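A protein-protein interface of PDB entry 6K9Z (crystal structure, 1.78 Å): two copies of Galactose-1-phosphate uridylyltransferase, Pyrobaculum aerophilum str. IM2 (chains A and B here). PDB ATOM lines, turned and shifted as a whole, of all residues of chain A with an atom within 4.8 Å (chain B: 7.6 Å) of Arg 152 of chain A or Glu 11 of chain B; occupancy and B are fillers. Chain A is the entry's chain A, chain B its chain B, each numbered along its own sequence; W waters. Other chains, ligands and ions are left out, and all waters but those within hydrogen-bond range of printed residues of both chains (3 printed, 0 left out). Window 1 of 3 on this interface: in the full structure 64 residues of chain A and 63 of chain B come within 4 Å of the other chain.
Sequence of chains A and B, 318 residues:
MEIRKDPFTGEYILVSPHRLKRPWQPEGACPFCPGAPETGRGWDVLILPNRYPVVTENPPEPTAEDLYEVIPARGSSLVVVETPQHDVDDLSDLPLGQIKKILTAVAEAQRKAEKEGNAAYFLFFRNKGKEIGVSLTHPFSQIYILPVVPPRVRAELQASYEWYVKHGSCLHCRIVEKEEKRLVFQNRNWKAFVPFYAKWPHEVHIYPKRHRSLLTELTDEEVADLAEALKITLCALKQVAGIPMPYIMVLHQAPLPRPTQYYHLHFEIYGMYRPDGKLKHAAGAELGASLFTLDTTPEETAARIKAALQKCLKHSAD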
ATOM      1  N   PRO A 150     -13.637 -19.313   5.178  1.00  0.00           N
ATOM      2  CA  PRO A 150     -14.388 -18.325   4.400  1.00  0.00           C
ATOM      3  C   PRO A 150     -15.184 -18.935   3.244  1.00  0.00           C
ATOM      4  O   PRO A 150     -14.655 -19.793   2.513  1.00  0.00           O
ATOM      5  CB  PRO A 150     -13.278 -17.447   3.864  1.00  0.00           C
ATOM      6  CG  PRO A 150     -12.172 -17.536   4.897  1.00  0.00           C
ATOM      7  CD  PRO A 150     -12.211 -18.990   5.343  1.00  0.00           C
ATOM      8  N   PRO A 151     -16.482 -18.566   3.060  1.00  0.00           N
ATOM      9  CA  PRO A 151     -17.323 -19.238   2.068  1.00  0.00           C
ATOM     10  C   PRO A 151     -16.743 -19.286   0.648  1.00  0.00           C
ATOM     11  O   PRO A 151     -16.893 -20.328   0.010  1.00  0.00           O
ATOM     12  CB  PRO A 151     -18.667 -18.488   2.130  1.00  0.00           C
ATOM     13  CG  PRO A 151     -18.717 -18.074   3.595  1.00  0.00           C
ATOM     14  CD  PRO A 151     -17.289 -17.675   3.928  1.00  0.00           C
ATOM     15  N   ARG A 152     -16.069 -18.230   0.194  1.00  0.00           N
ATOM     16  CA  ARG A 152     -15.555 -18.227  -1.199  1.00  0.00           C
ATOM     17  C   ARG A 152     -14.450 -19.282  -1.319  1.00  0.00           C
ATOM     18  O   ARG A 152     -14.405 -20.011  -2.295  1.00  0.00           O
ATOM     19  CB  ARG A 152     -15.042 -16.847  -1.596  1.00  0.00           C
ATOM     20  CG  ARG A 152     -14.392 -16.825  -2.983  1.00  0.00           C
ATOM     21  CD  ARG A 152     -14.077 -15.460  -3.601  1.00  0.00           C
ATOM     22  NE  ARG A 152     -15.346 -14.869  -3.849  1.00  0.00           N
ATOM     23  CZ  ARG A 152     -16.099 -15.128  -4.884  1.00  0.00           C
ATOM     24  NH1 ARG A 152     -15.655 -15.871  -5.864  1.00  0.00           N
ATOM     25  NH2 ARG A 152     -17.291 -14.568  -4.972  1.00  0.00           N
ATOM     26  N   VAL A 153     -13.636 -19.405  -0.271  1.00  0.00           N
ATOM     27  CA  VAL A 153     -12.541 -20.412  -0.264  1.00  0.00           C
ATOM     28  C   VAL A 153     -13.147 -21.798  -0.099  1.00  0.00           C
ATOM     29  O   VAL A 153     -12.688 -22.691  -0.814  1.00  0.00           O
ATOM     30  CB  VAL A 153     -11.457 -20.100   0.791  1.00  0.00           C
ATOM     31  CG1 VAL A 153     -10.398 -21.221   0.817  1.00  0.00           C
ATOM     32  CG2 VAL A 153     -10.844 -18.721   0.498  1.00  0.00           C
ATOM     33  N   ARG A 154     -14.196 -21.967   0.710  1.00  0.00           N
ATOM     34  CA  ARG A 154     -14.884 -23.268   0.836  1.00  0.00           C
ATOM     35  C   ARG A 154     -15.348 -23.708  -0.557  1.00  0.00           C
ATOM     36  O   ARG A 154     -15.215 -24.899  -0.858  1.00  0.00           O
ATOM     37  CB  ARG A 154     -16.081 -23.224   1.778  1.00  0.00           C
ATOM     38  CG  ARG A 154     -16.785 -24.568   1.977  1.00  0.00           C
ATOM     39  CD  ARG A 154     -17.876 -24.500   3.036  1.00  0.00           C
ATOM     40  NE  ARG A 154     -17.438 -24.468   4.465  1.00  0.00           N
ATOM     41  CZ  ARG A 154     -17.290 -23.348   5.260  1.00  0.00           C
ATOM     42  NH1 ARG A 154     -17.460 -22.126   4.769  1.00  0.00           N
ATOM     43  NH2 ARG A 154     -16.959 -23.478   6.552  1.00  0.00           N
ATOM     44  N   ALA A 155     -16.016 -22.837  -1.320  1.00  0.00           N
ATOM     45  CA  ALA A 155     -16.541 -23.186  -2.667  1.00  0.00           C
ATOM     46  C   ALA A 155     -15.337 -23.645  -3.527  1.00  0.00           C
ATOM     47  O   ALA A 155     -15.426 -24.702  -4.199  1.00  0.00           O
ATOM     48  CB  ALA A 155     -17.246 -22.002  -3.275  1.00  0.00           C
ATOM     49  N   GLU A 156     -14.206 -22.929  -3.445  1.00  0.00           N
ATOM     50  CA  GLU A 156     -13.035 -23.250  -4.299  1.00  0.00           C
ATOM     51  C   GLU A 156     -12.471 -24.615  -3.863  1.00  0.00           C
ATOM     52  O   GLU A 156     -12.077 -25.417  -4.749  1.00  0.00           O
ATOM     53  CB  GLU A 156     -11.950 -22.191  -4.223  1.00  0.00           C
ATOM     54  CG  GLU A 156     -12.321 -20.774  -4.669  1.00  0.00           C
ATOM     55  CD  GLU A 156     -11.163 -19.861  -5.020  1.00  0.00           C
ATOM     56  OE1 GLU A 156      -9.966 -20.272  -4.803  1.00  0.00           O
ATOM     57  OE2 GLU A 156     -11.414 -18.743  -5.530  1.00  0.00           O
ATOM     58  N   LYS A 199     -13.300 -11.547 -13.134  1.00  0.00           N
ATOM     59  CA  LYS A 199     -14.599 -10.885 -12.817  1.00  0.00           C
ATOM     60  C   LYS A 199     -14.444  -9.385 -12.604  1.00  0.00           C
ATOM     61  O   LYS A 199     -15.458  -8.625 -12.707  1.00  0.00           O
ATOM     62  CB  LYS A 199     -15.122 -11.381 -11.473  1.00  0.00           C
ATOM     63  CG  LYS A 199     -15.557 -12.802 -11.449  1.00  0.00           C
ATOM     64  CD  LYS A 199     -15.640 -13.319 -10.029  1.00  0.00           C
ATOM     65  CE  LYS A 199     -15.542 -14.822 -10.077  1.00  0.00           C
ATOM     66  NZ  LYS A 199     -14.307 -15.263 -10.778  1.00  0.00           N
ATOM     67  N   HIS A 252      -5.757 -16.886  -1.099  1.00  0.00           N
ATOM     68  CA  HIS A 252      -6.585 -18.116  -1.100  1.00  0.00           C
ATOM     69  C   HIS A 252      -5.608 -19.259  -0.825  1.00  0.00           C
ATOM     70  O   HIS A 252      -4.783 -19.537  -1.705  1.00  0.00           O
ATOM     71  CB  HIS A 252      -7.284 -18.244  -2.446  1.00  0.00           C
ATOM     72  CG  HIS A 252      -8.449 -17.334  -2.576  1.00  0.00           C
ATOM     73  ND1 HIS A 252      -9.236 -17.310  -3.717  1.00  0.00           N
ATOM     74  CD2 HIS A 252      -9.009 -16.499  -1.675  1.00  0.00           C
ATOM     75  CE1 HIS A 252     -10.224 -16.447  -3.515  1.00  0.00           C
ATOM     76  NE2 HIS A 252     -10.129 -15.910  -2.288  1.00  0.00           N
ATOM     77  N   TYR A 270      -7.706  -7.667  -7.278  1.00  0.00           N
ATOM     78  CA  TYR A 270      -8.852  -7.037  -7.971  1.00  0.00           C
ATOM     79  C   TYR A 270      -8.533  -5.559  -8.071  1.00  0.00           C
ATOM     80  O   TYR A 270      -8.708  -4.894  -7.099  1.00  0.00           O
ATOM     81  CB  TYR A 270     -10.154  -7.288  -7.237  1.00  0.00           C
ATOM     82  CG  TYR A 270     -10.392  -8.681  -6.735  1.00  0.00           C
ATOM     83  CD1 TYR A 270      -9.966  -9.808  -7.399  1.00  0.00           C
ATOM     84  CD2 TYR A 270     -11.144  -8.853  -5.587  1.00  0.00           C
ATOM     85  CE1 TYR A 270     -10.263 -11.084  -6.946  1.00  0.00           C
ATOM     86  CE2 TYR A 270     -11.435 -10.110  -5.079  1.00  0.00           C
ATOM     87  CZ  TYR A 270     -10.956 -11.238  -5.752  1.00  0.00           C
ATOM     88  OH  TYR A 270     -11.248 -12.466  -5.229  1.00  0.00           O
ATOM     89  N   SER A 290     -24.431 -12.569  -7.490  1.00  0.00           N
ATOM     90  CA  SER A 290     -23.094 -13.160  -7.771  1.00  0.00           C
ATOM     91  C   SER A 290     -22.903 -13.286  -9.277  1.00  0.00           C
ATOM     92  O   SER A 290     -22.407 -14.337  -9.718  1.00  0.00           O
ATOM     93  CB  SER A 290     -22.863 -14.521  -7.116  1.00  0.00           C
ATOM     94  OG  SER A 290     -22.914 -14.355  -5.742  1.00  0.00           O
ATOM     95  N   PHE A 292     -21.216 -11.260 -12.611  1.00  0.00           N
ATOM     96  CA  PHE A 292     -20.177 -10.267 -12.892  1.00  0.00           C
ATOM     97  C   PHE A 292     -20.199  -9.930 -14.410  1.00  0.00           C
ATOM     98  O   PHE A 292     -20.638 -10.770 -15.262  1.00  0.00           O
ATOM     99  CB  PHE A 292     -18.858 -10.858 -12.431  1.00  0.00           C
ATOM    100  CG  PHE A 292     -18.922 -11.322 -11.006  1.00  0.00           C
ATOM    101  CD1 PHE A 292     -19.330 -12.593 -10.686  1.00  0.00           C
ATOM    102  CD2 PHE A 292     -18.616 -10.445  -9.984  1.00  0.00           C
ATOM    103  CE1 PHE A 292     -19.443 -12.996  -9.360  1.00  0.00           C
ATOM    104  CE2 PHE A 292     -18.723 -10.849  -8.670  1.00  0.00           C
ATOM    105  CZ  PHE A 292     -19.124 -12.125  -8.361  1.00  0.00           C
ATOM    106  N   ILE B   3     -20.749 -15.784 -22.024  1.00  0.00           N
ATOM    107  CA  ILE B   3     -20.797 -16.028 -20.556  1.00  0.00           C
ATOM    108  C   ILE B   3     -19.709 -17.060 -20.210  1.00  0.00           C
ATOM    109  O   ILE B   3     -19.753 -18.194 -20.759  1.00  0.00           O
ATOM    110  CB  ILE B   3     -22.190 -16.458 -20.145  1.00  0.00           C
ATOM    111  CG1 ILE B   3     -23.195 -15.338 -20.434  1.00  0.00           C
ATOM    112  CG2 ILE B   3     -22.195 -16.889 -18.686  1.00  0.00           C
ATOM    113  CD1 ILE B   3     -24.620 -15.713 -20.201  1.00  0.00           C
ATOM    114  N   ARG B   4     -18.725 -16.635 -19.416  1.00  0.00           N
ATOM    115  CA  ARG B   4     -17.625 -17.500 -18.943  1.00  0.00           C
ATOM    116  C   ARG B   4     -17.989 -18.018 -17.560  1.00  0.00           C
ATOM    117  O   ARG B   4     -18.793 -17.400 -16.897  1.00  0.00           O
ATOM    118  CB  ARG B   4     -16.299 -16.753 -18.923  1.00  0.00           C
ATOM    119  CG  ARG B   4     -15.914 -16.183 -20.274  1.00  0.00           C
ATOM    120  CD  ARG B   4     -14.560 -15.570 -20.305  1.00  0.00           C
ATOM    121  NE  ARG B   4     -14.201 -15.075 -21.617  1.00  0.00           N
ATOM    122  CZ  ARG B   4     -12.988 -14.759 -22.014  1.00  0.00           C
ATOM    123  NH1 ARG B   4     -11.928 -14.901 -21.202  1.00  0.00           N
ATOM    124  NH2 ARG B   4     -12.818 -14.307 -23.246  1.00  0.00           N
ATOM    125  N   LYS B   5     -17.414 -19.145 -17.160  1.00  0.00           N
ATOM    126  CA  LYS B   5     -17.794 -19.774 -15.880  1.00  0.00           C
ATOM    127  C   LYS B   5     -16.497 -20.002 -15.100  1.00  0.00           C
ATOM    128  O   LYS B   5     -15.521 -20.500 -15.675  1.00  0.00           O
ATOM    129  CB  LYS B   5     -18.560 -21.089 -16.040  1.00  0.00           C
ATOM    130  CG  LYS B   5     -19.103 -21.653 -14.737  1.00  0.00           C
ATOM    131  CD  LYS B   5     -19.686 -23.086 -14.884  1.00  0.00           C
ATOM    132  CE  LYS B   5     -20.661 -23.452 -13.783  1.00  0.00           C
ATOM    133  NZ  LYS B   5     -21.308 -24.780 -14.026  1.00  0.00           N
ATOM    134  N   ASP B   6     -16.469 -19.528 -13.847  1.00  0.00           N
ATOM    135  CA  ASP B   6     -15.334 -19.786 -12.920  1.00  0.00           C
ATOM    136  C   ASP B   6     -15.409 -21.255 -12.513  1.00  0.00           C
ATOM    137  O   ASP B   6     -16.408 -21.691 -11.914  1.00  0.00           O
ATOM    138  CB  ASP B   6     -15.443 -18.853 -11.734  1.00  0.00           C
ATOM    139  CG  ASP B   6     -14.319 -18.920 -10.716  1.00  0.00           C
ATOM    140  OD1 ASP B   6     -13.903 -20.012 -10.411  1.00  0.00           O
ATOM    141  OD2 ASP B   6     -13.983 -17.857 -10.174  1.00  0.00           O
ATOM    142  N   PRO B   7     -14.347 -22.006 -12.734  1.00  0.00           N
ATOM    143  CA  PRO B   7     -14.374 -23.444 -12.496  1.00  0.00           C
ATOM    144  C   PRO B   7     -14.295 -23.779 -10.997  1.00  0.00           C
ATOM    145  O   PRO B   7     -14.523 -24.917 -10.626  1.00  0.00           O
ATOM    146  CB  PRO B   7     -13.207 -23.921 -13.333  1.00  0.00           C
ATOM    147  CG  PRO B   7     -12.217 -22.799 -13.290  1.00  0.00           C
ATOM    148  CD  PRO B   7     -13.066 -21.553 -13.308  1.00  0.00           C
ATOM    149  N   PHE B   8     -13.936 -22.807 -10.172  1.00  0.00           N
ATOM    150  CA  PHE B   8     -13.754 -23.024  -8.705  1.00  0.00           C
ATOM    151  C   PHE B   8     -15.010 -22.595  -7.947  1.00  0.00           C
ATOM    152  O   PHE B   8     -15.223 -23.088  -6.849  1.00  0.00           O
ATOM    153  CB  PHE B   8     -12.489 -22.314  -8.215  1.00  0.00           C
ATOM    154  CG  PHE B   8     -11.230 -22.812  -8.867  1.00  0.00           C
ATOM    155  CD1 PHE B   8     -10.761 -24.105  -8.637  1.00  0.00           C
ATOM    156  CD2 PHE B   8     -10.545 -22.026  -9.773  1.00  0.00           C
ATOM    157  CE1 PHE B   8      -9.625 -24.589  -9.277  1.00  0.00           C
ATOM    158  CE2 PHE B   8      -9.374 -22.486 -10.361  1.00  0.00           C
ATOM    159  CZ  PHE B   8      -8.941 -23.784 -10.160  1.00  0.00           C
ATOM    160  N   THR B   9     -15.831 -21.686  -8.485  1.00  0.00           N
ATOM    161  CA  THR B   9     -17.002 -21.152  -7.753  1.00  0.00           C
ATOM    162  C   THR B   9     -18.306 -21.433  -8.493  1.00  0.00           C
ATOM    163  O   THR B   9     -19.335 -21.337  -7.864  1.00  0.00           O
ATOM    164  CB  THR B   9     -16.871 -19.656  -7.476  1.00  0.00           C
ATOM    165  OG1 THR B   9     -16.848 -18.988  -8.751  1.00  0.00           O
ATOM    166  CG2 THR B   9     -15.651 -19.270  -6.656  1.00  0.00           C
ATOM    167  N   GLY B  10     -18.265 -21.653  -9.796  1.00  0.00           N
ATOM    168  CA  GLY B  10     -19.487 -21.711 -10.630  1.00  0.00           C
ATOM    169  C   GLY B  10     -20.025 -20.360 -10.973  1.00  0.00           C
ATOM    170  O   GLY B  10     -21.151 -20.291 -11.481  1.00  0.00           O
ATOM    171  N   GLU B  11     -19.310 -19.299 -10.603  1.00  0.00           N
ATOM    172  CA  GLU B  11     -19.789 -17.927 -10.904  1.00  0.00           C
ATOM    173  C   GLU B  11     -19.706 -17.683 -12.410  1.00  0.00           C
ATOM    174  O   GLU B  11     -18.806 -18.238 -13.046  1.00  0.00           O
ATOM    175  CB  GLU B  11     -19.016 -16.892 -10.093  1.00  0.00           C
ATOM    176  CG  GLU B  11     -19.289 -17.006  -8.610  1.00  0.00           C
ATOM    177  CD  GLU B  11     -18.330 -16.205  -7.757  1.00  0.00           C
ATOM    178  OE1 GLU B  11     -17.115 -16.319  -7.981  1.00  0.00           O
ATOM    179  OE2 GLU B  11     -18.807 -15.460  -6.888  1.00  0.00           O
ATOM    180  N   TYR B  12     -20.624 -16.868 -12.931  1.00  0.00           N
ATOM    181  CA  TYR B  12     -20.684 -16.554 -14.379  1.00  0.00           C
ATOM    182  C   TYR B  12     -20.239 -15.111 -14.602  1.00  0.00           C
ATOM    183  O   TYR B  12     -20.613 -14.232 -13.812  1.00  0.00           O
ATOM    184  CB  TYR B  12     -22.115 -16.692 -14.899  1.00  0.00           C
ATOM    185  CG  TYR B  12     -22.677 -18.086 -14.847  1.00  0.00           C
ATOM    186  CD1 TYR B  12     -22.188 -19.088 -15.667  1.00  0.00           C
ATOM    187  CD2 TYR B  12     -23.705 -18.401 -13.978  1.00  0.00           C
ATOM    188  CE1 TYR B  12     -22.708 -20.370 -15.622  1.00  0.00           C
ATOM    189  CE2 TYR B  12     -24.236 -19.675 -13.923  1.00  0.00           C
ATOM    190  CZ  TYR B  12     -23.737 -20.664 -14.746  1.00  0.00           C
ATOM    191  OH  TYR B  12     -24.262 -21.916 -14.691  1.00  0.00           O
ATOM    192  N   ILE B  13     -19.422 -14.898 -15.632  1.00  0.00           N
ATOM    193  CA  ILE B  13     -18.971 -13.523 -15.975  1.00  0.00           C
ATOM    194  C   ILE B  13     -19.579 -13.179 -17.335  1.00  0.00           C
ATOM    195  O   ILE B  13     -19.318 -13.918 -18.294  1.00  0.00           O
ATOM    196  CB  ILE B  13     -17.433 -13.438 -16.003  1.00  0.00           C
ATOM    197  CG1 ILE B  13     -16.805 -14.059 -14.753  1.00  0.00           C
ATOM    198  CG2 ILE B  13     -16.984 -12.000 -16.200  1.00  0.00           C
ATOM    199  CD1 ILE B  13     -16.651 -15.559 -14.817  1.00  0.00           C
ATOM    200  N   LEU B  14     -20.357 -12.099 -17.410  1.00  0.00           N
ATOM    201  CA  LEU B  14     -20.929 -11.708 -18.722  1.00  0.00           C
ATOM    202  C   LEU B  14     -19.868 -10.829 -19.378  1.00  0.00           C
ATOM    203  O   LEU B  14     -19.768  -9.648 -19.030  1.00  0.00           O
ATOM    204  CB  LEU B  14     -22.245 -10.954 -18.506  1.00  0.00           C
ATOM    205  CG  LEU B  14     -23.234 -11.616 -17.547  1.00  0.00           C
ATOM    206  CD1 LEU B  14     -24.590 -10.936 -17.608  1.00  0.00           C
ATOM    207  CD2 LEU B  14     -23.374 -13.099 -17.834  1.00  0.00           C
ATOM    208  N   GLU B  69     -15.672 -23.689 -19.322  1.00  0.00           N
ATOM    209  CA  GLU B  69     -17.064 -23.723 -19.827  1.00  0.00           C
ATOM    210  C   GLU B  69     -17.456 -22.314 -20.244  1.00  0.00           C
ATOM    211  O   GLU B  69     -17.390 -21.393 -19.388  1.00  0.00           O
ATOM    212  CB  GLU B  69     -18.032 -24.272 -18.780  1.00  0.00           C
ATOM    213  CG  GLU B  69     -17.710 -25.688 -18.330  1.00  0.00           C
ATOM    214  CD  GLU B  69     -18.768 -26.247 -17.393  1.00  0.00           C
ATOM    215  OE1 GLU B  69     -19.882 -26.552 -17.900  1.00  0.00           O
ATOM    216  OE2 GLU B  69     -18.520 -26.300 -16.163  1.00  0.00           O
ATOM    217  N   PRO B 150     -28.670 -17.032 -11.761  1.00  0.00           N
ATOM    218  CA  PRO B 150     -27.657 -16.322 -10.961  1.00  0.00           C
ATOM    219  C   PRO B 150     -27.094 -17.156  -9.812  1.00  0.00           C
ATOM    220  O   PRO B 150     -27.838 -17.854  -9.108  1.00  0.00           O
ATOM    221  CB  PRO B 150     -28.473 -15.220 -10.382  1.00  0.00           C
ATOM    222  CG  PRO B 150     -29.449 -14.901 -11.487  1.00  0.00           C
ATOM    223  CD  PRO B 150     -29.893 -16.251 -11.988  1.00  0.00           C
ATOM    224  N   PRO B 151     -25.760 -17.278  -9.680  1.00  0.00           N
ATOM    225  CA  PRO B 151     -25.221 -18.204  -8.680  1.00  0.00           C
ATOM    226  C   PRO B 151     -25.693 -18.022  -7.228  1.00  0.00           C
ATOM    227  O   PRO B 151     -25.848 -19.008  -6.497  1.00  0.00           O
ATOM    228  CB  PRO B 151     -23.712 -17.984  -8.821  1.00  0.00           C
ATOM    229  CG  PRO B 151     -23.524 -17.555 -10.268  1.00  0.00           C
ATOM    230  CD  PRO B 151     -24.755 -16.747 -10.610  1.00  0.00           C
ATOM    231  N   ARG B 152     -25.935 -16.776  -6.821  1.00  0.00           N
ATOM    232  CA  ARG B 152     -26.486 -16.528  -5.467  1.00  0.00           C
ATOM    233  C   ARG B 152     -27.879 -17.165  -5.337  1.00  0.00           C
ATOM    234  O   ARG B 152     -28.179 -17.789  -4.309  1.00  0.00           O
ATOM    235  CB  ARG B 152     -26.659 -15.038  -5.157  1.00  0.00           C
ATOM    236  CG  ARG B 152     -27.205 -14.804  -3.739  1.00  0.00           C
ATOM    237  CD  ARG B 152     -27.036 -13.355  -3.264  1.00  0.00           C
ATOM    238  NE  ARG B 152     -25.615 -13.142  -2.998  1.00  0.00           N
ATOM    239  CZ  ARG B 152     -24.980 -13.521  -1.887  1.00  0.00           C
ATOM    240  NH1 ARG B 152     -25.631 -14.101  -0.894  1.00  0.00           N
ATOM    241  NH2 ARG B 152     -23.676 -13.318  -1.760  1.00  0.00           N
ATOM    242  N   ARG B 154     -28.922 -19.669  -7.150  1.00  0.00           N
ATOM    243  CA  ARG B 154     -28.743 -21.145  -7.212  1.00  0.00           C
ATOM    244  C   ARG B 154     -28.430 -21.681  -5.810  1.00  0.00           C
ATOM    245  O   ARG B 154     -28.999 -22.714  -5.443  1.00  0.00           O
ATOM    246  CB  ARG B 154     -27.621 -21.530  -8.179  1.00  0.00           C
ATOM    247  CG  ARG B 154     -27.467 -23.033  -8.353  1.00  0.00           C
ATOM    248  CD  ARG B 154     -26.486 -23.387  -9.450  1.00  0.00           C
ATOM    249  NE  ARG B 154     -27.083 -23.373 -10.776  1.00  0.00           N
ATOM    250  CZ  ARG B 154     -26.988 -22.365 -11.634  1.00  0.00           C
ATOM    251  NH1 ARG B 154     -26.321 -21.272 -11.304  1.00  0.00           N
ATOM    252  NH2 ARG B 154     -27.564 -22.453 -12.820  1.00  0.00           N
ATOM    253  N   GLY B 284     -11.980  -6.612   0.443  1.00  0.00           N
ATOM    254  CA  GLY B 284     -11.287  -7.909   0.575  1.00  0.00           C
ATOM    255  C   GLY B 284     -12.073  -8.980   1.312  1.00  0.00           C
ATOM    256  O   GLY B 284     -12.133 -10.103   0.787  1.00  0.00           O
ATOM    257  N   ALA B 285     -12.686  -8.663   2.458  1.00  0.00           N
ATOM    258  CA  ALA B 285     -13.452  -9.693   3.161  1.00  0.00           C
ATOM    259  C   ALA B 285     -14.652 -10.120   2.320  1.00  0.00           C
ATOM    260  O   ALA B 285     -14.891 -11.338   2.108  1.00  0.00           O
ATOM    261  CB  ALA B 285     -13.864  -9.211   4.537  1.00  0.00           C
ATOM    262  N   GLU B 286     -15.405  -9.150   1.755  1.00  0.00           N
ATOM    263  CA  GLU B 286     -16.666  -9.488   1.076  1.00  0.00           C
ATOM    264  C   GLU B 286     -16.373 -10.090  -0.306  1.00  0.00           C
ATOM    265  O   GLU B 286     -16.967 -11.097  -0.618  1.00  0.00           O
ATOM    266  CB  GLU B 286     -17.535  -8.220   0.924  1.00  0.00           C
ATOM    267  CG  GLU B 286     -17.865  -7.614   2.307  1.00  0.00           C
ATOM    268  CD  GLU B 286     -16.830  -6.676   2.919  1.00  0.00           C
ATOM    269  OE1 GLU B 286     -15.760  -6.406   2.316  1.00  0.00           O
ATOM    270  OE2 GLU B 286     -17.094  -6.135   4.033  1.00  0.00           O
ATOM    271  N   LEU B 287     -15.615  -9.407  -1.117  1.00  0.00           N
ATOM    272  CA  LEU B 287     -15.368  -9.798  -2.532  1.00  0.00           C
ATOM    273  C   LEU B 287     -14.314 -10.924  -2.558  1.00  0.00           C
ATOM    274  O   LEU B 287     -14.476 -11.866  -3.389  1.00  0.00           O
ATOM    275  CB  LEU B 287     -14.877  -8.636  -3.358  1.00  0.00           C
ATOM    276  CG  LEU B 287     -15.820  -7.426  -3.397  1.00  0.00           C
ATOM    277  CD1 LEU B 287     -15.296  -6.380  -4.351  1.00  0.00           C
ATOM    278  CD2 LEU B 287     -17.224  -7.876  -3.751  1.00  0.00           C
ATOM    279  N   GLY B 288     -13.326 -10.815  -1.696  1.00  0.00           N
ATOM    280  CA  GLY B 288     -12.208 -11.801  -1.603  1.00  0.00           C
ATOM    281  C   GLY B 288     -12.623 -13.093  -0.948  1.00  0.00           C
ATOM    282  O   GLY B 288     -12.009 -14.191  -1.272  1.00  0.00           O
ATOM    283  N   ALA B 289     -13.500 -13.066   0.066  1.00  0.00           N
ATOM    284  CA  ALA B 289     -13.678 -14.230   0.953  1.00  0.00           C
ATOM    285  C   ALA B 289     -15.159 -14.606   1.149  1.00  0.00           C
ATOM    286  O   ALA B 289     -15.453 -15.615   1.783  1.00  0.00           O
ATOM    287  CB  ALA B 289     -12.977 -13.961   2.229  1.00  0.00           C
ATOM    288  N   SER B 290     -16.083 -13.780   0.654  1.00  0.00           N
ATOM    289  CA  SER B 290     -17.534 -13.920   0.973  1.00  0.00           C
ATOM    290  C   SER B 290     -17.714 -13.956   2.478  1.00  0.00           C
ATOM    291  O   SER B 290     -18.608 -14.698   2.972  1.00  0.00           O
ATOM    292  CB  SER B 290     -18.252 -15.086   0.308  1.00  0.00           C
ATOM    293  OG  SER B 290     -18.119 -14.967  -1.085  1.00  0.00           O
ATOM    294  N   LEU B 291     -16.976 -13.104   3.186  1.00  0.00           N
ATOM    295  CA  LEU B 291     -17.111 -12.846   4.627  1.00  0.00           C
ATOM    296  C   LEU B 291     -17.658 -11.437   4.852  1.00  0.00           C
ATOM    297  O   LEU B 291     -17.154 -10.507   4.232  1.00  0.00           O
ATOM    298  CB  LEU B 291     -15.763 -12.828   5.332  1.00  0.00           C
ATOM    299  CG  LEU B 291     -15.227 -14.107   5.911  1.00  0.00           C
ATOM    300  CD1 LEU B 291     -13.955 -13.752   6.673  1.00  0.00           C
ATOM    301  CD2 LEU B 291     -16.199 -14.860   6.793  1.00  0.00           C
HETATM  302  O   HOH W   1     -13.944 -12.500  -6.709  1.00  0.00           O
HETATM  303  O   HOH W   2     -16.246 -11.721  -5.688  1.00  0.00           O
HETATM  304  O   HOH W   3     -23.082 -12.123  -4.418  1.00  0.00           O
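OE2 of Glu 11 of chain B is in salt-bridge range of NH2 of Arg 152 of chain A, 2.6 Å away.
The guanidinium group (NE) of Arg 152 of chain A is in hydrogen-bond range of the backbone carbonyl oxygen (O) of Leu 287 of chain B (3.2 Å).
N of Arg 152 of chain A is in hydrogen-bond range of O of Ala 289 of chain B.
NZ of Lys 199 of chain A lies within salt-bridge range of OD2 of Asp 6 of chain B (2.7 Å).
A ring nitrogen (NE2) of His 252 of chain A is in hydrogen-bond range of the backbone carbonyl oxygen of Gly 288 of chain B (2.7 Å).
O of Tyr 12 of chain B lies within hydrogen-bond range of N of Phe 292 of chain A (3.3 Å).
The backbone carbonyl oxygen of Phe 292 of chain A sits at hydrogen-bond distance from the backbone NH of Leu 14 of chain B.
The backbone nitrogen (N) of Pro 151 of chain A lies close to the backbone carbonyl oxygen (O) of Ala 289 of chain B (3.4 Å).
O of Phe 8 of chain B lies close to O of Ala 155 of chain A.
O of Gly 284 of chain B is in hydrogen-bond range of N of Ala 289 of chain B, at 3.3 Å.
N of Ser 290 of chain B lies within hydrogen-bond range of O of Ala 285 of chain B (3.1 Å).
Pro 151 of chain A touches Ser 290 of chain B (CD to O, 3.4 Å).
Arg 152 of chain A touches Gly 288 of chain B.
Ser 290 of chain B touches Arg 152 of chain A.
Tyr 270 of chain A touches Leu 287 of chain B (OH to O, 3.8 Å).
Phe 292 of chain A touches Ile 13 of chain B (O to CA, 3.3 Å).
Printed residues of chain B within 4 Å of Pro 150 of chain A: Ala 289.
Arg 152 of chain A touches six residues of chain B.
Of the printed residues of chain A, Ile 13 of chain B touches Lys 199 (3.7 Å) and Phe 292 (3.3 Å).
The nearest printed residue of chain A that does not touch Ser 290 of chain B is Pro 150 of chain A (5.5 Å).
Along chain B the printed residues that touch a printed residue of chain A span positions 6 to 290.
Of the 12 printed residues of chain A, 10 touch a printed residue of chain B.
Hydrophobic or aromatic side chains of chain A within 4 Å of the printed part of chain B: Pro 150, Pro 151, His 252, Tyr 270 and Phe 292.
Among the printed residues, 23 pairs touch across the chains.
Pro 151 of chain A touches Ser 290 of chain B, and with the chains exchanged Ser 290 of chain A touches Pro 151 of chain B.
Arg 152 of chain A touches Ser 290 of chain B, and with the chains exchanged Ser 290 of chain A touches Arg 152 of chain B.
Positions printed for both chains: 150, 151, 152, 154 and 290.
Water W3 lies within hydrogen-bond range of the side-chain hydroxyl (OG) of Ser 290 of chain A and the guanidinium group (NH2) of Arg 152 of chain B.
Water W2 bridges O of Leu 287 of chain B and NH2 of Arg 152 of chain A.
Water W1 bridges OH of Tyr 270 of chain A (3.1 Å) and O of Leu 287 of chain B (3.4 Å).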
